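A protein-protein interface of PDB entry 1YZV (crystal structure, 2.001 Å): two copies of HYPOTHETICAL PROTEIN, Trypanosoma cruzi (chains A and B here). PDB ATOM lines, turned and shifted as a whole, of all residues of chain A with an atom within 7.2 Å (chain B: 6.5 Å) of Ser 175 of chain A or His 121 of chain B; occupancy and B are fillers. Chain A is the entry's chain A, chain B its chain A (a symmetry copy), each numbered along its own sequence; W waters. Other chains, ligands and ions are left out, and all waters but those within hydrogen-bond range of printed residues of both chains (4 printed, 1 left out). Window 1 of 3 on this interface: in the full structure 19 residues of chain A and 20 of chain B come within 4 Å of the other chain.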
ATOM      1  N   LEU A  12     -21.814  24.537   3.717  1.00  0.00           N
ATOM      2  CA  LEU A  12     -22.722  24.556   4.840  1.00  0.00           C
ATOM      3  C   LEU A  12     -23.916  25.417   4.463  1.00  0.00           C
ATOM      4  O   LEU A  12     -23.893  26.081   3.416  1.00  0.00           O
ATOM      5  CB  LEU A  12     -22.016  25.146   6.049  1.00  0.00           C
ATOM      6  CG  LEU A  12     -20.831  24.332   6.609  1.00  0.00           C
ATOM      7  CD1 LEU A  12     -20.159  25.125   7.671  1.00  0.00           C
ATOM      8  CD2 LEU A  12     -21.275  22.975   7.095  1.00  0.00           C
ATOM      9  N   LEU A  13     -24.933  25.446   5.332  1.00  0.00           N
ATOM     10  CA  LEU A  13     -26.067  26.345   5.141  1.00  0.00           C
ATOM     11  C   LEU A  13     -25.535  27.776   5.058  1.00  0.00           C
ATOM     12  O   LEU A  13     -24.556  28.118   5.710  1.00  0.00           O
ATOM     13  CB  LEU A  13     -27.031  26.243   6.318  1.00  0.00           C
ATOM     14  CG  LEU A  13     -27.812  24.936   6.424  1.00  0.00           C
ATOM     15  CD1 LEU A  13     -28.389  24.815   7.815  1.00  0.00           C
ATOM     16  CD2 LEU A  13     -28.908  24.869   5.365  1.00  0.00           C
ATOM     17  N   ARG A  48     -37.404  23.116  18.697  1.00  0.00           N
ATOM     18  CA  ARG A  48     -36.252  23.972  18.553  1.00  0.00           C
ATOM     19  C   ARG A  48     -36.306  24.749  17.239  1.00  0.00           C
ATOM     20  O   ARG A  48     -36.050  25.971  17.186  1.00  0.00           O
ATOM     21  CB  ARG A  48     -34.985  23.103  18.621  1.00  0.00           C
ATOM     22  CG  ARG A  48     -33.736  23.822  18.242  1.00  0.00           C
ATOM     23  CD  ARG A  48     -32.516  23.000  18.596  1.00  0.00           C
ATOM     24  NE  ARG A  48     -32.228  23.032  20.022  1.00  0.00           N
ATOM     25  CZ  ARG A  48     -31.177  22.433  20.579  1.00  0.00           C
ATOM     26  NH1 ARG A  48     -30.316  21.726  19.820  1.00  0.00           N
ATOM     27  NH2 ARG A  48     -30.922  22.630  21.868  1.00  0.00           N
ATOM     28  N   ASP A 143     -30.291  14.298  14.948  1.00  0.00           N
ATOM     29  CA  ASP A 143     -30.821  14.233  16.324  1.00  0.00           C
ATOM     30  C   ASP A 143     -32.337  14.376  16.407  1.00  0.00           C
ATOM     31  O   ASP A 143     -32.917  13.992  17.424  1.00  0.00           O
ATOM     32  CB  ASP A 143     -30.122  15.244  17.306  1.00  0.00           C
ATOM     33  CG  ASP A 143     -30.203  16.737  16.859  1.00  0.00           C
ATOM     34  OD1 ASP A 143     -30.053  17.010  15.655  1.00  0.00           O
ATOM     35  OD2 ASP A 143     -30.299  17.651  17.744  1.00  0.00           O
ATOM     36  N   TYR A 169     -26.116  17.004   3.230  1.00  0.00           N
ATOM     37  CA  TYR A 169     -25.310  16.492   4.336  1.00  0.00           C
ATOM     38  C   TYR A 169     -26.041  16.369   5.661  1.00  0.00           C
ATOM     39  O   TYR A 169     -27.208  16.784   5.816  1.00  0.00           O
ATOM     40  CB  TYR A 169     -24.109  17.357   4.525  1.00  0.00           C
ATOM     41  CG  TYR A 169     -24.445  18.724   4.991  1.00  0.00           C
ATOM     42  CD1 TYR A 169     -24.627  19.748   4.066  1.00  0.00           C
ATOM     43  CD2 TYR A 169     -24.259  19.087   6.359  1.00  0.00           C
ATOM     44  CE1 TYR A 169     -24.866  21.041   4.496  1.00  0.00           C
ATOM     45  CE2 TYR A 169     -24.493  20.375   6.801  1.00  0.00           C
ATOM     46  CZ  TYR A 169     -24.873  21.350   5.869  1.00  0.00           C
ATOM     47  OH  TYR A 169     -25.027  22.688   6.264  1.00  0.00           O
ATOM     48  N   SER A 171     -26.186  16.822   9.728  1.00  0.00           N
ATOM     49  CA  SER A 171     -25.720  17.677  10.823  1.00  0.00           C
ATOM     50  C   SER A 171     -26.626  17.465  12.035  1.00  0.00           C
ATOM     51  O   SER A 171     -27.313  16.435  12.137  1.00  0.00           O
ATOM     52  CB  SER A 171     -25.677  19.149  10.351  1.00  0.00           C
ATOM     53  OG  SER A 171     -24.945  19.979  11.237  1.00  0.00           O
ATOM     54  N   THR A 172     -26.443  18.292  13.057  1.00  0.00           N
ATOM     55  CA  THR A 172     -27.316  18.254  14.254  1.00  0.00           C
ATOM     56  C   THR A 172     -28.000  19.600  14.405  1.00  0.00           C
ATOM     57  O   THR A 172     -27.463  20.608  13.983  1.00  0.00           O
ATOM     58  CB  THR A 172     -26.539  17.899  15.544  1.00  0.00           C
ATOM     59  OG1 THR A 172     -25.481  18.833  15.729  1.00  0.00           O
ATOM     60  CG2 THR A 172     -25.977  16.490  15.474  1.00  0.00           C
ATOM     61  N   SER A 173     -29.112  19.637  15.150  1.00  0.00           N
ATOM     62  CA  SER A 173     -29.890  20.879  15.307  1.00  0.00           C
ATOM     63  C   SER A 173     -29.071  22.052  15.863  1.00  0.00           C
ATOM     64  O   SER A 173     -29.168  23.200  15.373  1.00  0.00           O
ATOM     65  CB  SER A 173     -31.161  20.606  16.145  1.00  0.00           C
ATOM     66  OG  SER A 173     -30.858  20.173  17.499  1.00  0.00           O
ATOM     67  N   GLU A 174     -28.172  21.776  16.802  1.00  0.00           N
ATOM     68  CA  GLU A 174     -27.399  22.869  17.378  1.00  0.00           C
ATOM     69  C   GLU A 174     -26.398  23.450  16.351  1.00  0.00           C
ATOM     70  O   GLU A 174     -26.273  24.672  16.221  1.00  0.00           O
ATOM     71  CB  GLU A 174     -26.672  22.416  18.653  1.00  0.00           C
ATOM     72  CG  GLU A 174     -25.998  23.574  19.330  1.00  0.00           C
ATOM     73  CD  GLU A 174     -25.475  23.223  20.695  1.00  0.00           C
ATOM     74  OE1 GLU A 174     -26.293  23.155  21.646  1.00  0.00           O
ATOM     75  OE2 GLU A 174     -24.250  23.064  20.785  1.00  0.00           O
ATOM     76  N   SER A 175     -25.795  22.565  15.563  1.00  0.00           N
ATOM     77  CA  SER A 175     -24.882  22.936  14.524  1.00  0.00           C
ATOM     78  C   SER A 175     -25.601  23.719  13.449  1.00  0.00           C
ATOM     79  O   SER A 175     -25.131  24.790  13.070  1.00  0.00           O
ATOM     80  CB  SER A 175     -24.224  21.720  13.928  1.00  0.00           C
ATOM     81  OG  SER A 175     -23.135  22.083  13.118  1.00  0.00           O
ATOM     82  N   ILE A 176     -26.826  23.285  13.162  1.00  0.00           N
ATOM     83  CA  ILE A 176     -27.676  23.921  12.151  1.00  0.00           C
ATOM     84  C   ILE A 176     -28.055  25.360  12.580  1.00  0.00           C
ATOM     85  O   ILE A 176     -27.839  26.324  11.814  1.00  0.00           O
ATOM     86  CB  ILE A 176     -28.881  23.047  11.849  1.00  0.00           C
ATOM     87  CG1 ILE A 176     -28.434  21.817  11.056  1.00  0.00           C
ATOM     88  CG2 ILE A 176     -30.019  23.808  11.154  1.00  0.00           C
ATOM     89  CD1 ILE A 176     -29.404  20.657  11.107  1.00  0.00           C
ATOM     90  N   LEU A 177     -28.476  25.521  13.836  1.00  0.00           N
ATOM     91  CA  LEU A 177     -28.775  26.846  14.347  1.00  0.00           C
ATOM     92  C   LEU A 177     -27.602  27.813  14.132  1.00  0.00           C
ATOM     93  O   LEU A 177     -27.787  28.957  13.655  1.00  0.00           O
ATOM     94  CB  LEU A 177     -29.159  26.770  15.836  1.00  0.00           C
ATOM     95  CG  LEU A 177     -30.626  26.808  16.154  1.00  0.00           C
ATOM     96  CD1 LEU A 177     -31.361  25.661  15.471  1.00  0.00           C
ATOM     97  CD2 LEU A 177     -30.851  26.812  17.664  1.00  0.00           C
ATOM     98  N   MET A 178     -26.405  27.374  14.517  1.00  0.00           N
ATOM     99  CA  MET A 178     -25.214  28.229  14.514  1.00  0.00           C
ATOM    100  C   MET A 178     -24.647  28.421  13.098  1.00  0.00           C
ATOM    101  O   MET A 178     -24.093  29.479  12.800  1.00  0.00           O
ATOM    102  CB  MET A 178     -24.165  27.654  15.481  1.00  0.00           C
ATOM    103  CG  MET A 178     -24.662  27.595  16.927  1.00  0.00           C
ATOM    104  SD  MET A 178     -24.963  29.234  17.571  1.00  0.00           S
ATOM    105  CE  MET A 178     -26.705  29.537  17.246  1.00  0.00           C
ATOM    106  N   GLN A 179     -24.921  27.464  12.200  1.00  0.00           N
ATOM    107  CA  GLN A 179     -24.673  27.641  10.748  1.00  0.00           C
ATOM    108  C   GLN A 179     -25.488  28.767  10.109  1.00  0.00           C
ATOM    109  O   GLN A 179     -24.978  29.524   9.265  1.00  0.00           O
ATOM    110  CB  GLN A 179     -24.927  26.349   9.949  1.00  0.00           C
ATOM    111  CG  GLN A 179     -23.862  25.288  10.140  1.00  0.00           C
ATOM    112  CD  GLN A 179     -24.323  23.918   9.595  1.00  0.00           C
ATOM    113  OE1 GLN A 179     -24.839  23.847   8.504  1.00  0.00           O
ATOM    114  NE2 GLN A 179     -24.168  22.870  10.385  1.00  0.00           N
ATOM    115  N   LEU A 180     -26.744  28.878  10.506  1.00  0.00           N
ATOM    116  CA  LEU A 180     -27.632  29.892   9.953  1.00  0.00           C
ATOM    117  C   LEU A 180     -27.261  31.268  10.471  1.00  0.00           C
ATOM    118  O   LEU A 180     -27.587  32.230   9.825  1.00  0.00           O
ATOM    119  CB  LEU A 180     -29.094  29.595  10.263  1.00  0.00           C
ATOM    120  CG  LEU A 180     -29.641  28.410   9.502  1.00  0.00           C
ATOM    121  CD1 LEU A 180     -30.886  27.813  10.222  1.00  0.00           C
ATOM    122  CD2 LEU A 180     -29.929  28.810   8.028  1.00  0.00           C
ATOM    123  N   LEU A 181     -26.750  31.352  11.709  1.00  0.00           N
ATOM    124  CA  LEU A 181     -26.398  32.628  12.334  1.00  0.00           C
ATOM    125  C   LEU A 181     -24.985  33.150  12.095  1.00  0.00           C
ATOM    126  O   LEU A 181     -24.783  34.374  12.094  1.00  0.00           O
ATOM    127  CB  LEU A 181     -26.656  32.596  13.836  1.00  0.00           C
ATOM    128  CG  LEU A 181     -28.063  32.958  14.311  1.00  0.00           C
ATOM    129  CD1 LEU A 181     -29.159  32.172  13.599  1.00  0.00           C
ATOM    130  CD2 LEU A 181     -28.090  32.639  15.728  1.00  0.00           C
ATOM    131  N   MET A 196     -30.572  26.893  22.547  1.00  0.00           N
ATOM    132  CA  MET A 196     -29.441  25.993  22.685  1.00  0.00           C
ATOM    133  C   MET A 196     -29.101  25.589  24.088  1.00  0.00           C
ATOM    134  O   MET A 196     -28.458  24.573  24.270  1.00  0.00           O
ATOM    135  CB  MET A 196     -28.226  26.589  22.025  1.00  0.00           C
ATOM    136  CG  MET A 196     -28.281  26.306  20.550  1.00  0.00           C
ATOM    137  SD  MET A 196     -27.044  27.247  19.776  1.00  0.00           S
ATOM    138  CE  MET A 196     -25.544  26.847  20.659  1.00  0.00           C
ATOM    139  N   PHE B 118     -12.568  23.990  20.440  1.00  0.00           N
ATOM    140  CA  PHE B 118     -13.976  23.992  20.799  1.00  0.00           C
ATOM    141  C   PHE B 118     -14.765  24.991  19.921  1.00  0.00           C
ATOM    142  O   PHE B 118     -14.238  26.020  19.529  1.00  0.00           O
ATOM    143  CB  PHE B 118     -14.202  24.444  22.220  1.00  0.00           C
ATOM    144  CG  PHE B 118     -13.397  23.708  23.284  1.00  0.00           C
ATOM    145  CD1 PHE B 118     -13.112  22.377  23.189  1.00  0.00           C
ATOM    146  CD2 PHE B 118     -13.194  24.352  24.512  1.00  0.00           C
ATOM    147  CE1 PHE B 118     -12.437  21.733  24.242  1.00  0.00           C
ATOM    148  CE2 PHE B 118     -12.518  23.722  25.554  1.00  0.00           C
ATOM    149  CZ  PHE B 118     -12.102  22.428  25.394  1.00  0.00           C
ATOM    150  N   GLU B 119     -16.031  24.699  19.619  1.00  0.00           N
ATOM    151  CA  GLU B 119     -16.640  23.389  19.724  1.00  0.00           C
ATOM    152  C   GLU B 119     -16.590  22.809  18.305  1.00  0.00           C
ATOM    153  O   GLU B 119     -16.644  23.563  17.323  1.00  0.00           O
ATOM    154  CB  GLU B 119     -18.102  23.490  20.197  1.00  0.00           C
ATOM    155  CG  GLU B 119     -18.243  23.872  21.653  1.00  0.00           C
ATOM    156  CD  GLU B 119     -19.661  23.669  22.210  1.00  0.00           C
ATOM    157  OE1 GLU B 119     -20.178  22.538  22.266  1.00  0.00           O
ATOM    158  OE2 GLU B 119     -20.241  24.663  22.633  1.00  0.00           O
ATOM    159  N   THR B 120     -16.487  21.491  18.216  1.00  0.00           N
ATOM    160  CA  THR B 120     -16.315  20.769  16.933  1.00  0.00           C
ATOM    161  C   THR B 120     -17.362  21.153  15.877  1.00  0.00           C
ATOM    162  O   THR B 120     -17.023  21.410  14.737  1.00  0.00           O
ATOM    163  CB  THR B 120     -16.315  19.248  17.162  1.00  0.00           C
ATOM    164  OG1 THR B 120     -15.445  18.928  18.262  1.00  0.00           O
ATOM    165  CG2 THR B 120     -15.828  18.489  15.912  1.00  0.00           C
ATOM    166  N   HIS B 121     -18.628  21.262  16.294  1.00  0.00           N
ATOM    167  CA  HIS B 121     -19.749  21.471  15.402  1.00  0.00           C
ATOM    168  C   HIS B 121     -20.083  22.923  15.173  1.00  0.00           C
ATOM    169  O   HIS B 121     -21.038  23.252  14.451  1.00  0.00           O
ATOM    170  CB  HIS B 121     -20.985  20.726  15.918  1.00  0.00           C
ATOM    171  CG  HIS B 121     -21.489  21.217  17.235  1.00  0.00           C
ATOM    172  ND1 HIS B 121     -20.718  21.197  18.374  1.00  0.00           N
ATOM    173  CD2 HIS B 121     -22.679  21.779  17.590  1.00  0.00           C
ATOM    174  CE1 HIS B 121     -21.381  21.788  19.354  1.00  0.00           C
ATOM    175  NE2 HIS B 121     -22.600  22.075  18.928  1.00  0.00           N
ATOM    176  N   VAL B 122     -19.338  23.811  15.818  1.00  0.00           N
ATOM    177  CA  VAL B 122     -19.574  25.259  15.654  1.00  0.00           C
ATOM    178  C   VAL B 122     -18.353  26.003  15.128  1.00  0.00           C
ATOM    179  O   VAL B 122     -18.098  26.040  13.923  1.00  0.00           O
ATOM    180  CB  VAL B 122     -20.153  25.901  16.941  1.00  0.00           C
ATOM    181  CG1 VAL B 122     -20.470  27.406  16.739  1.00  0.00           C
ATOM    182  CG2 VAL B 122     -21.450  25.174  17.329  1.00  0.00           C
ATOM    183  N   CYS B 123     -17.484  26.435  16.018  1.00  0.00           N
ATOM    184  CA  CYS B 123     -16.304  27.185  15.583  1.00  0.00           C
ATOM    185  C   CYS B 123     -15.307  26.384  14.733  1.00  0.00           C
ATOM    186  O   CYS B 123     -14.801  26.874  13.718  1.00  0.00           O
ATOM    187  CB  CYS B 123     -15.675  27.897  16.815  1.00  0.00           C
ATOM    188  SG  CYS B 123     -16.891  29.213  17.564  1.00  0.00           S
ATOM    189  N   ILE B 124     -15.060  25.120  15.075  1.00  0.00           N
ATOM    190  CA  ILE B 124     -14.164  24.324  14.295  1.00  0.00           C
ATOM    191  C   ILE B 124     -14.731  24.036  12.896  1.00  0.00           C
ATOM    192  O   ILE B 124     -14.040  24.199  11.895  1.00  0.00           O
ATOM    193  CB  ILE B 124     -13.851  22.970  14.968  1.00  0.00           C
ATOM    194  CG1 ILE B 124     -13.292  23.194  16.356  1.00  0.00           C
ATOM    195  CG2 ILE B 124     -12.982  22.074  14.052  1.00  0.00           C
ATOM    196  CD1 ILE B 124     -11.929  23.498  16.356  1.00  0.00           C
ATOM    197  N   LEU B 125     -15.933  23.491  12.848  1.00  0.00           N
ATOM    198  CA  LEU B 125     -16.618  23.252  11.608  1.00  0.00           C
ATOM    199  C   LEU B 125     -16.626  24.471  10.676  1.00  0.00           C
ATOM    200  O   LEU B 125     -16.359  24.334   9.475  1.00  0.00           O
ATOM    201  CB  LEU B 125     -18.062  22.837  11.881  1.00  0.00           C
ATOM    202  CG  LEU B 125     -18.908  22.488  10.653  1.00  0.00           C
ATOM    203  CD1 LEU B 125     -18.313  21.322   9.915  1.00  0.00           C
ATOM    204  CD2 LEU B 125     -20.382  22.223  11.012  1.00  0.00           C
ATOM    205  N   GLN B 126     -17.125  25.599  11.177  1.00  0.00           N
ATOM    206  CA  GLN B 126     -17.213  26.802  10.375  1.00  0.00           C
ATOM    207  C   GLN B 126     -15.850  27.379   9.923  1.00  0.00           C
ATOM    208  O   GLN B 126     -15.741  27.935   8.843  1.00  0.00           O
ATOM    209  CB  GLN B 126     -18.080  27.890  11.057  1.00  0.00           C
ATOM    210  CG  GLN B 126     -19.489  27.369  11.326  1.00  0.00           C
ATOM    211  CD  GLN B 126     -20.478  28.401  11.706  1.00  0.00           C
ATOM    212  OE1 GLN B 126     -20.365  29.581  11.317  1.00  0.00           O
ATOM    213  NE2 GLN B 126     -21.487  27.978  12.473  1.00  0.00           N
ATOM    214  N   GLY B 146     -13.572  18.961  20.630  1.00  0.00           N
ATOM    215  CA  GLY B 146     -14.636  18.546  21.491  1.00  0.00           C
ATOM    216  C   GLY B 146     -15.840  19.435  21.404  1.00  0.00           C
ATOM    217  O   GLY B 146     -15.713  20.632  21.010  1.00  0.00           O
ATOM    218  N   SER B 147     -16.981  18.879  21.835  1.00  0.00           N
ATOM    219  CA  SER B 147     -18.237  19.630  21.934  1.00  0.00           C
ATOM    220  C   SER B 147     -18.865  19.354  23.287  1.00  0.00           C
ATOM    221  O   SER B 147     -18.456  18.420  23.994  1.00  0.00           O
ATOM    222  CB  SER B 147     -19.251  19.240  20.832  1.00  0.00           C
ATOM    223  OG  SER B 147     -18.752  19.469  19.535  1.00  0.00           O
ATOM    224  N   GLN B 148     -19.894  20.124  23.640  1.00  0.00           N
ATOM    225  CA  GLN B 148     -20.577  19.853  24.916  1.00  0.00           C
ATOM    226  C   GLN B 148     -21.364  18.533  24.862  1.00  0.00           C
ATOM    227  O   GLN B 148     -21.547  17.859  25.883  1.00  0.00           O
ATOM    228  CB  GLN B 148     -21.453  21.041  25.331  1.00  0.00           C
ATOM    229  CG  GLN B 148     -20.612  22.273  25.715  1.00  0.00           C
ATOM    230  CD  GLN B 148     -21.433  23.454  26.170  1.00  0.00           C
ATOM    231  OE1 GLN B 148     -21.541  24.453  25.456  1.00  0.00           O
ATOM    232  NE2 GLN B 148     -22.228  23.229  27.189  1.00  0.00           N
ATOM    233  N   SER B 149     -21.728  18.069  23.670  1.00  0.00           N
ATOM    234  CA  SER B 149     -22.327  16.769  23.567  1.00  0.00           C
ATOM    235  C   SER B 149     -21.569  15.918  22.575  1.00  0.00           C
ATOM    236  O   SER B 149     -21.121  16.406  21.539  1.00  0.00           O
ATOM    237  CB  SER B 149     -23.788  16.897  23.134  1.00  0.00           C
ATOM    238  OG  SER B 149     -23.957  16.332  21.833  1.00  0.00           O
ATOM    239  N   ASP B 152     -23.142  15.928  18.906  1.00  0.00           N
ATOM    240  CA  ASP B 152     -22.790  17.111  18.133  1.00  0.00           C
ATOM    241  C   ASP B 152     -21.368  16.998  17.557  1.00  0.00           C
ATOM    242  O   ASP B 152     -21.118  17.299  16.403  1.00  0.00           O
ATOM    243  CB  ASP B 152     -22.916  18.401  18.960  1.00  0.00           C
ATOM    244  CG  ASP B 152     -24.388  18.798  19.213  1.00  0.00           C
ATOM    245  OD1 ASP B 152     -25.297  18.499  18.370  1.00  0.00           O
ATOM    246  OD2 ASP B 152     -24.668  19.241  20.343  1.00  0.00           O
ATOM    247  N   HIS B 153     -20.448  16.522  18.375  1.00  0.00           N
ATOM    248  CA  HIS B 153     -19.051  16.390  17.954  1.00  0.00           C
ATOM    249  C   HIS B 153     -18.924  15.337  16.870  1.00  0.00           C
ATOM    250  O   HIS B 153     -18.308  15.602  15.835  1.00  0.00           O
ATOM    251  CB  HIS B 153     -18.220  16.019  19.211  1.00  0.00           C
ATOM    252  CG  HIS B 153     -16.891  15.441  18.906  1.00  0.00           C
ATOM    253  ND1 HIS B 153     -15.783  16.236  18.681  1.00  0.00           N
ATOM    254  CD2 HIS B 153     -16.507  14.169  18.660  1.00  0.00           C
ATOM    255  CE1 HIS B 153     -14.744  15.456  18.454  1.00  0.00           C
ATOM    256  NE2 HIS B 153     -15.157  14.201  18.421  1.00  0.00           N
ATOM    257  N   THR B 155     -21.020  13.823  14.772  1.00  0.00           N
ATOM    258  CA  THR B 155     -21.699  14.153  13.506  1.00  0.00           C
ATOM    259  C   THR B 155     -20.945  15.189  12.692  1.00  0.00           C
ATOM    260  O   THR B 155     -20.720  14.979  11.478  1.00  0.00           O
ATOM    261  CB  THR B 155     -23.120  14.632  13.761  1.00  0.00           C
ATOM    262  OG1 THR B 155     -23.819  13.605  14.456  1.00  0.00           O
ATOM    263  CG2 THR B 155     -23.876  14.937  12.447  1.00  0.00           C
ATOM    264  N   ALA B 156     -20.354  16.174  13.371  1.00  0.00           N
ATOM    265  CA  ALA B 156     -19.524  17.164  12.712  1.00  0.00           C
ATOM    266  C   ALA B 156     -18.176  16.632  12.201  1.00  0.00           C
ATOM    267  O   ALA B 156     -17.711  17.000  11.119  1.00  0.00           O
ATOM    268  CB  ALA B 156     -19.314  18.345  13.605  1.00  0.00           C
ATOM    269  N   LEU B 159     -19.050  14.883   9.145  1.00  0.00           N
ATOM    270  CA  LEU B 159     -19.296  15.849   8.061  1.00  0.00           C
ATOM    271  C   LEU B 159     -17.966  16.295   7.407  1.00  0.00           C
ATOM    272  O   LEU B 159     -17.778  16.177   6.184  1.00  0.00           O
ATOM    273  CB  LEU B 159     -20.077  17.042   8.601  1.00  0.00           C
ATOM    274  CG  LEU B 159     -20.419  18.207   7.661  1.00  0.00           C
ATOM    275  CD1 LEU B 159     -20.861  17.694   6.303  1.00  0.00           C
ATOM    276  CD2 LEU B 159     -21.534  18.991   8.374  1.00  0.00           C
ATOM    277  N   MET B 160     -17.003  16.671   8.242  1.00  0.00           N
ATOM    278  CA  MET B 160     -15.698  17.064   7.777  1.00  0.00           C
ATOM    279  C   MET B 160     -14.923  15.952   7.073  1.00  0.00           C
ATOM    280  O   MET B 160     -14.276  16.228   6.073  1.00  0.00           O
ATOM    281  CB  MET B 160     -14.888  17.662   8.900  1.00  0.00           C
ATOM    282  CG  MET B 160     -15.473  18.940   9.349  1.00  0.00           C
ATOM    283  SD  MET B 160     -14.550  19.889  10.550  1.00  0.00           S
ATOM    284  CE  MET B 160     -14.871  18.994  12.039  1.00  0.00           C
HETATM  285  O   HOH W   1     -22.936  20.257  22.062  1.00  0.00           O
HETATM  286  O   HOH W   2     -22.358  25.440  13.322  1.00  0.00           O
HETATM  287  O   HOH W   3     -27.901  19.278  18.544  1.00  0.00           O
HETATM  288  O   HOH W   4     -23.060  18.270  14.592  1.00  0.00           O
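No position is printed for both chains. Of the 12 pairs that touch across the chains among the printed residues, none has its exchanged pair printed and touching as well.
The backbone carbonyl oxygen (O) of Thr 120 of chain B sits at hydrogen-bond distance from the backbone NH (N) of Leu 125 of chain B. The side-chain hydroxyl (OH) of Tyr 169 of chain A sits at hydrogen-bond distance from the backbone NH (N) of Leu 13 of chain A, 2.9 Å away. The side-chain hydroxyl (OG) of Ser 171 of chain A lies close to the side-chain hydroxyl (OG) of Ser 175 of chain A (3.4 Å). The side-chain hydroxyl (OG) of Ser 149 of chain B sits at hydrogen-bond distance from the backbone NH (N) of Asp 152 of chain B, at 3.1 Å. ND1 of His 121 of chain B sits at hydrogen-bond distance from OG of Ser 147 of chain B (2.9 Å). NE2 of Gln 179 of chain A lies within hydrogen-bond range of OG of Ser 175 of chain A (3.0 Å).
The side-chain carboxylate (OE2) of Glu 174 of chain A lies within hydrogen-bond range of a ring nitrogen (NE2) of His 121 of chain B (2.7 Å). The side-chain carboxylate of Asp 152 of chain B is in hydrogen-bond range of the side-chain hydroxyl of Thr 172 of chain A, 2.7 Å away. N of Gln 179 of chain A lies close to NE2 of Gln 126 of chain B (3.5 Å). NE2 of Gln 126 of chain B is in hydrogen-bond range of O of Met 178 of chain A (3.0 Å). The backbone carbonyl oxygen of His 121 of chain B sits at hydrogen-bond distance from the side-chain hydroxyl of Ser 175 of chain A (2.7 Å).
Printed residues of chain A that touch a printed residue of chain B: Tyr 169, Ser 171, Thr 172, Glu 174, Ser 175, Met 178 and Gln 179. Hydrophobic or aromatic side chains of chain A within 4 Å of the printed part of chain B: Tyr 169 and Met 178. Of the 19 printed residues of chain B, 7 touch a printed residue of chain A. Printed residues of chain B that touch a printed residue of chain A: His 121, Val 122, Leu 125, Gln 126, Asp 152, Thr 155 and Leu 159. Along chain B the printed residues that touch a printed residue of chain A span positions 121 to 159. Among the printed residues, no Asp or Glu carboxylate lies within 4 Å of a Lys or Arg side-chain nitrogen of the other chain.
Printed residues of chain B within 4 Å of Tyr 169 of chain A: Leu 159. Printed residues of chain B within 4 Å of Glu 174 of chain A: His 121 (2.7 Å) and Asp 152 (3.9 Å). Of chain B, only His 121 and Leu 125 come within 4 Å of Ser 175 of chain A. His 121 of chain B touches just these residues of chain A: Glu 174 and Ser 175. Of the printed residues of chain A, Thr 155 of chain B touches Ser 171 and Thr 172. Of the printed residues of chain A, Leu 159 of chain B touches Tyr 169. The nearest residue of chain B that does not touch Ser 175 of chain A is Gln 126 of chain B (4.9 Å). The nearest printed residue of chain B that does not touch Glu 174 of chain A is Glu 119 of chain B (4.4 Å).
Tyr 169 of chain A touches Leu 159 of chain B (CD2 to CD2, 3.4 Å). CG2 of Thr 155 of chain B touches CA of Ser 171 of chain A, 3.7 Å away. Thr 155 of chain B touches Thr 172 of chain A. Asp 152 of chain B touches Glu 174 of chain A. Ser 175 of chain A touches Leu 125 of chain B. Met 178 of chain A touches Val 122 of chain B (CB to CG1, 3.9 Å). Gln 179 of chain A touches Leu 125 of chain B (NE2 to CD2, 3.9 Å).
Water W1 lies within hydrogen-bond range of the side-chain carboxylate (OD2) of Asp 152 of chain B, the backbone NH (N) of Ser 149 of chain B, the side-chain carboxylate (OE2) of Glu 174 of chain A and the backbone NH (N) of Gln 148 of chain B. Water W3 lies within hydrogen-bond range of the side-chain carboxylate of Asp 152 of chain B (2.7 Å), the side-chain carboxylate of Asp 143 of chain A (3.0 Å), the backbone NH of Glu 174 of chain A (3.1 Å) and the side-chain hydroxyl of Ser 173 of chain A (3.3 Å). Water W4 lies within hydrogen-bond range of OG1 of Thr 172 of chain A (2.7 Å) and O of Asp 152 of chain B (2.8 Å). Water W2 lies within hydrogen-bond range of the backbone carbonyl oxygen (O) of His 121 of chain B (2.8 Å), the side-chain amide nitrogen (NE2) of Gln 126 of chain B (2.8 Å), the backbone carbonyl oxygen (O) of Ser 175 of chain A (2.9 Å) and the backbone NH (N) of Gln 179 of chain A (3.5 Å).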
